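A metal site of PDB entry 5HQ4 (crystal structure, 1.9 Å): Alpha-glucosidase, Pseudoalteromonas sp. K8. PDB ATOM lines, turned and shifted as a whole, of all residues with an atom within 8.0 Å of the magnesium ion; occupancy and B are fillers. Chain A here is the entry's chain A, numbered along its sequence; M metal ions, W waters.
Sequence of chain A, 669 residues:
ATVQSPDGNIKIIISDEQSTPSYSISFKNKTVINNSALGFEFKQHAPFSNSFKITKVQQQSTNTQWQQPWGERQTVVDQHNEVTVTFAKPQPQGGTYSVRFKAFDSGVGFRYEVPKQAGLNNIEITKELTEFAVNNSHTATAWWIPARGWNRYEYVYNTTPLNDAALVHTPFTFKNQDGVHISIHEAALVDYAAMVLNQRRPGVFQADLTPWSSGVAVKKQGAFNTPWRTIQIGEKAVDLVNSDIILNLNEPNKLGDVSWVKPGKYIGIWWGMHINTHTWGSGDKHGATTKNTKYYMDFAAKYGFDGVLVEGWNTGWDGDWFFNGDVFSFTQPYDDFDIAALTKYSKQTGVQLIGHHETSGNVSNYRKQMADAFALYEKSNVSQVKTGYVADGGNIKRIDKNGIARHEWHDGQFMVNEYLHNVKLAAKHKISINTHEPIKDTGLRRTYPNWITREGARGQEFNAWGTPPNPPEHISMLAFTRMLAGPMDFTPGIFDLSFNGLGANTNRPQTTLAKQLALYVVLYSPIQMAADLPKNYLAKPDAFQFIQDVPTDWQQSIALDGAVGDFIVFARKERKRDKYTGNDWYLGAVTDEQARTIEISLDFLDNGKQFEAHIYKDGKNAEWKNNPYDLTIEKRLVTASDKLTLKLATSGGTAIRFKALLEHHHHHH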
ATOM      1  N   TRP A 143       0.259 -11.152  10.906  1.00  0.00           N
ATOM      2  CA  TRP A 143      -0.649 -10.068  11.248  1.00  0.00           C
ATOM      3  C   TRP A 143      -2.043 -10.670  11.347  1.00  0.00           C
ATOM      4  O   TRP A 143      -2.596 -11.100  10.327  1.00  0.00           O
ATOM      5  CB  TRP A 143      -0.606  -8.970  10.170  1.00  0.00           C
ATOM      6  CG  TRP A 143       0.777  -8.432   9.906  1.00  0.00           C
ATOM      7  CD1 TRP A 143       1.413  -7.445  10.596  1.00  0.00           C
ATOM      8  CD2 TRP A 143       1.676  -8.856   8.874  1.00  0.00           C
ATOM      9  NE1 TRP A 143       2.655  -7.209  10.045  1.00  0.00           N
ATOM     10  CE2 TRP A 143       2.840  -8.074   8.995  1.00  0.00           C
ATOM     11  CE3 TRP A 143       1.610  -9.810   7.853  1.00  0.00           C
ATOM     12  CZ2 TRP A 143       3.929  -8.213   8.126  1.00  0.00           C
ATOM     13  CZ3 TRP A 143       2.685  -9.949   6.987  1.00  0.00           C
ATOM     14  CH2 TRP A 143       3.832  -9.153   7.131  1.00  0.00           C
ATOM     15  N   THR A 159       0.556  -7.853  15.568  1.00  0.00           N
ATOM     16  CA  THR A 159       1.783  -8.068  14.794  1.00  0.00           C
ATOM     17  C   THR A 159       2.720  -8.873  15.676  1.00  0.00           C
ATOM     18  O   THR A 159       3.187  -8.364  16.689  1.00  0.00           O
ATOM     19  CB  THR A 159       2.439  -6.728  14.423  1.00  0.00           C
ATOM     20  OG1 THR A 159       1.502  -5.895  13.716  1.00  0.00           O
ATOM     21  CG2 THR A 159       3.722  -6.962  13.578  1.00  0.00           C
ATOM     22  N   PRO A 472      -3.906   4.148  14.109  1.00  0.00           N
ATOM     23  CA  PRO A 472      -3.480   4.611  12.778  1.00  0.00           C
ATOM     24  C   PRO A 472      -3.146   3.484  11.801  1.00  0.00           C
ATOM     25  O   PRO A 472      -3.422   3.615  10.603  1.00  0.00           O
ATOM     26  CB  PRO A 472      -2.253   5.455  13.094  1.00  0.00           C
ATOM     27  CG  PRO A 472      -2.580   6.052  14.446  1.00  0.00           C
ATOM     28  CD  PRO A 472      -3.288   4.941  15.193  1.00  0.00           C
ATOM     29  N   GLU A 473      -2.567   2.382  12.264  1.00  0.00           N
ATOM     30  CA  GLU A 473      -2.184   1.310  11.345  1.00  0.00           C
ATOM     31  C   GLU A 473      -3.377   0.494  10.827  1.00  0.00           C
ATOM     32  O   GLU A 473      -3.185  -0.367   9.971  1.00  0.00           O
ATOM     33  CB  GLU A 473      -1.183   0.367  12.027  1.00  0.00           C
ATOM     34  CG  GLU A 473      -1.809  -0.494  13.134  1.00  0.00           C
ATOM     35  CD  GLU A 473      -0.798  -1.405  13.829  1.00  0.00           C
ATOM     36  OE1 GLU A 473       0.414  -1.343  13.524  1.00  0.00           O
ATOM     37  OE2 GLU A 473      -1.225  -2.204  14.703  1.00  0.00           O
ATOM     38  N   HIS A 474      -4.597   0.747  11.330  1.00  0.00           N
ATOM     39  CA  HIS A 474      -5.691  -0.198  11.111  1.00  0.00           C
ATOM     40  C   HIS A 474      -5.994  -0.405   9.634  1.00  0.00           C
ATOM     41  O   HIS A 474      -6.152  -1.548   9.178  1.00  0.00           O
ATOM     42  CB  HIS A 474      -6.948   0.278  11.847  1.00  0.00           C
ATOM     43  CG  HIS A 474      -8.059  -0.728  11.832  1.00  0.00           C
ATOM     44  ND1 HIS A 474      -7.897  -2.030  12.285  1.00  0.00           N
ATOM     45  CD2 HIS A 474      -9.349  -0.630  11.424  1.00  0.00           C
ATOM     46  CE1 HIS A 474      -9.048  -2.677  12.156  1.00  0.00           C
ATOM     47  NE2 HIS A 474      -9.935  -1.854  11.636  1.00  0.00           N
ATOM     48  N   SER A 476      -4.112   0.044   6.987  1.00  0.00           N
ATOM     49  CA  SER A 476      -3.027  -0.689   6.327  1.00  0.00           C
ATOM     50  C   SER A 476      -2.919  -2.128   6.799  1.00  0.00           C
ATOM     51  O   SER A 476      -2.232  -2.920   6.143  1.00  0.00           O
ATOM     52  CB  SER A 476      -1.691   0.042   6.535  1.00  0.00           C
ATOM     53  OG  SER A 476      -1.294   0.003   7.902  1.00  0.00           O
ATOM     54  N   MET A 477      -3.569  -2.490   7.910  1.00  0.00           N
ATOM     55  CA  MET A 477      -3.738  -3.906   8.254  1.00  0.00           C
ATOM     56  C   MET A 477      -4.881  -4.523   7.462  1.00  0.00           C
ATOM     57  O   MET A 477      -4.706  -5.562   6.812  1.00  0.00           O
ATOM     58  CB  MET A 477      -4.003  -4.067   9.753  1.00  0.00           C
ATOM     59  CG  MET A 477      -2.828  -3.694  10.648  1.00  0.00           C
ATOM     60  SD  MET A 477      -1.481  -4.896  10.479  1.00  0.00           S
ATOM     61  CE  MET A 477      -0.374  -4.259  11.726  1.00  0.00           C
ATOM     62  N   ALA A 563       2.830  -2.253   2.155  1.00  0.00           N
ATOM     63  CA  ALA A 563       3.469  -3.149   3.112  1.00  0.00           C
ATOM     64  C   ALA A 563       2.500  -3.322   4.267  1.00  0.00           C
ATOM     65  O   ALA A 563       1.897  -2.349   4.721  1.00  0.00           O
ATOM     66  CB  ALA A 563       4.817  -2.585   3.614  1.00  0.00           C
ATOM     67  N   VAL A 564       2.351  -4.571   4.720  1.00  0.00           N
ATOM     68  CA  VAL A 564       1.290  -4.875   5.668  1.00  0.00           C
ATOM     69  C   VAL A 564       1.496  -4.071   6.943  1.00  0.00           C
ATOM     70  O   VAL A 564       2.580  -4.082   7.532  1.00  0.00           O
ATOM     71  CB  VAL A 564       1.238  -6.371   5.998  1.00  0.00           C
ATOM     72  CG1 VAL A 564       0.035  -6.635   6.913  1.00  0.00           C
ATOM     73  CG2 VAL A 564       1.185  -7.221   4.714  1.00  0.00           C
ATOM     74  N   GLY A 565       0.448  -3.385   7.376  1.00  0.00           N
ATOM     75  CA  GLY A 565       0.525  -2.608   8.595  1.00  0.00           C
ATOM     76  C   GLY A 565       1.309  -1.332   8.478  1.00  0.00           C
ATOM     77  O   GLY A 565       1.560  -0.682   9.506  1.00  0.00           O
ATOM     78  N   ASP A 566       1.711  -0.939   7.269  1.00  0.00           N
ATOM     79  CA  ASP A 566       2.454   0.298   7.041  1.00  0.00           C
ATOM     80  C   ASP A 566       1.776   1.226   6.053  1.00  0.00           C
ATOM     81  O   ASP A 566       1.554   2.401   6.380  1.00  0.00           O
ATOM     82  CB  ASP A 566       3.889   0.000   6.569  1.00  0.00           C
ATOM     83  CG  ASP A 566       4.760  -0.606   7.655  1.00  0.00           C
ATOM     84  OD1 ASP A 566       5.842  -1.124   7.328  1.00  0.00           O
ATOM     85  OD2 ASP A 566       4.353  -0.591   8.843  1.00  0.00           O
ATOM     86  N   PHE A 567       1.440   0.757   4.849  1.00  0.00           N
ATOM     87  CA  PHE A 567       0.807   1.637   3.859  1.00  0.00           C
ATOM     88  C   PHE A 567       0.268   0.816   2.705  1.00  0.00           C
ATOM     89  O   PHE A 567       0.636  -0.350   2.523  1.00  0.00           O
ATOM     90  CB  PHE A 567       1.797   2.701   3.341  1.00  0.00           C
ATOM     91  CG  PHE A 567       2.835   2.176   2.370  1.00  0.00           C
ATOM     92  CD1 PHE A 567       3.967   1.500   2.822  1.00  0.00           C
ATOM     93  CD2 PHE A 567       2.698   2.409   0.998  1.00  0.00           C
ATOM     94  CE1 PHE A 567       4.936   1.025   1.906  1.00  0.00           C
ATOM     95  CE2 PHE A 567       3.654   1.946   0.091  1.00  0.00           C
ATOM     96  CZ  PHE A 567       4.766   1.262   0.546  1.00  0.00           C
ATOM     97  N   THR A 591      -1.347   5.698   5.123  1.00  0.00           N
ATOM     98  CA  THR A 591      -0.223   5.226   5.915  1.00  0.00           C
ATOM     99  C   THR A 591      -0.717   4.855   7.310  1.00  0.00           C
ATOM    100  O   THR A 591      -1.886   5.021   7.654  1.00  0.00           O
ATOM    101  CB  THR A 591       0.874   6.284   5.970  1.00  0.00           C
ATOM    102  OG1 THR A 591       2.036   5.760   6.647  1.00  0.00           O
ATOM    103  CG2 THR A 591       0.359   7.539   6.729  1.00  0.00           C
ATOM    104  N   ASP A 592       0.215   4.350   8.118  1.00  0.00           N
ATOM    105  CA  ASP A 592      -0.038   3.972   9.509  1.00  0.00           C
ATOM    106  C   ASP A 592       0.307   5.149  10.408  1.00  0.00           C
ATOM    107  O   ASP A 592       0.086   6.294  10.034  1.00  0.00           O
ATOM    108  CB  ASP A 592       0.770   2.727   9.874  1.00  0.00           C
ATOM    109  CG  ASP A 592       2.281   2.923   9.673  1.00  0.00           C
ATOM    110  OD1 ASP A 592       3.062   1.960   9.871  1.00  0.00           O
ATOM    111  OD2 ASP A 592       2.688   4.041   9.313  1.00  0.00           O
ATOM    112  N   GLU A 593       0.899   4.903  11.586  1.00  0.00           N
ATOM    113  CA  GLU A 593       1.222   6.017  12.473  1.00  0.00           C
ATOM    114  C   GLU A 593       2.394   6.864  11.993  1.00  0.00           C
ATOM    115  O   GLU A 593       2.613   7.957  12.534  1.00  0.00           O
ATOM    116  CB  GLU A 593       1.510   5.495  13.892  1.00  0.00           C
ATOM    117  CG  GLU A 593       2.874   4.797  14.050  1.00  0.00           C
ATOM    118  CD  GLU A 593       2.890   3.387  13.452  1.00  0.00           C
ATOM    119  OE1 GLU A 593       3.992   2.830  13.306  1.00  0.00           O
ATOM    120  OE2 GLU A 593       1.809   2.844  13.135  1.00  0.00           O
ATOM    121  N   GLN A 594       3.141   6.406  10.989  1.00  0.00           N
ATOM    122  CA  GLN A 594       4.302   7.132  10.501  1.00  0.00           C
ATOM    123  C   GLN A 594       3.949   7.971   9.285  1.00  0.00           C
ATOM    124  O   GLN A 594       3.206   7.530   8.405  1.00  0.00           O
ATOM    125  CB  GLN A 594       5.433   6.166  10.139  1.00  0.00           C
ATOM    126  CG  GLN A 594       5.994   5.377  11.318  1.00  0.00           C
ATOM    127  CD  GLN A 594       7.259   4.609  10.945  1.00  0.00           C
ATOM    128  OE1 GLN A 594       7.798   4.776   9.852  1.00  0.00           O
ATOM    129  NE2 GLN A 594       7.731   3.767  11.861  1.00  0.00           N
ATOM    130  N   ARG A 596       4.948   9.161   5.700  1.00  0.00           N
ATOM    131  CA  ARG A 596       5.666   8.381   4.687  1.00  0.00           C
ATOM    132  C   ARG A 596       5.669   9.122   3.358  1.00  0.00           C
ATOM    133  O   ARG A 596       4.690   9.767   2.985  1.00  0.00           O
ATOM    134  CB  ARG A 596       5.051   6.977   4.478  1.00  0.00           C
ATOM    135  CG  ARG A 596       5.190   6.020   5.663  1.00  0.00           C
ATOM    136  CD  ARG A 596       4.576   4.605   5.426  1.00  0.00           C
ATOM    137  NE  ARG A 596       4.564   3.883   6.698  1.00  0.00           N
ATOM    138  CZ  ARG A 596       5.608   3.239   7.179  1.00  0.00           C
ATOM    139  NH1 ARG A 596       6.727   3.189   6.469  1.00  0.00           N
ATOM    140  NH2 ARG A 596       5.548   2.628   8.369  1.00  0.00           N
HETATM  141 MG    MG M   1       3.197  -0.042  10.512  1.00  0.00          MG
HETATM  142  O   HOH W   1       2.153   0.240  12.250  1.00  0.00           O
HETATM  143  O   HOH W   2       3.579  -1.932  11.193  1.00  0.00           O
HETATM  144  O   HOH W   3       4.821   0.706  11.573  1.00  0.00           O
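The backbone NH (N) of Gly 565 is in hydrogen-bond range of the backbone carbonyl oxygen (O) of Ser 476, 3.0 Å away. The guanidinium group (NH2) of Arg 596 lies within salt-bridge range of the side-chain carboxylate (OD1) of Asp 566 (3.9 Å). The backbone NH (N) of Asp 566 is in hydrogen-bond range of the side-chain hydroxyl (OG) of Ser 476 (3.2 Å). The backbone carbonyl oxygen (O) of Asp 566 lies close to the side-chain hydroxyl (OG1) of Thr 591, at 3.4 Å. NE of Arg 596 is in salt-bridge range of OD2 of Asp 592, 3.2 Å away. N of Gln 594 sits at hydrogen-bond distance from OD2 of Asp 592 (2.9 Å). The side-chain hydroxyl of Thr 591 sits at hydrogen-bond distance from the side-chain carboxylate of Asp 592 (3.2 Å).
Of the 17 residues printed, 3 come within 4 Å of the magnesium ion. Along chain A the residues within 4 Å of the magnesium ion span positions 565 to 592.
The magnesium ion is bound by O of Gly 565, at 2.0 Å. The magnesium ion is bound by water W2 (2.0 Å). Water W1 binds the magnesium ion (2.0 Å). The magnesium ion is bound by water W3, 2.1 Å away. OD2 of Asp 566 is bound to the magnesium ion (2.1 Å). The magnesium ion is bound by the side-chain carboxylate (OD1) of Asp 592 (2.1 Å). The magnesium ion has six donor atoms within binding distance.
Water W1 lies within hydrogen-bond range of the side-chain carboxylate of Glu 473 and the side-chain carboxylate of Glu 593.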
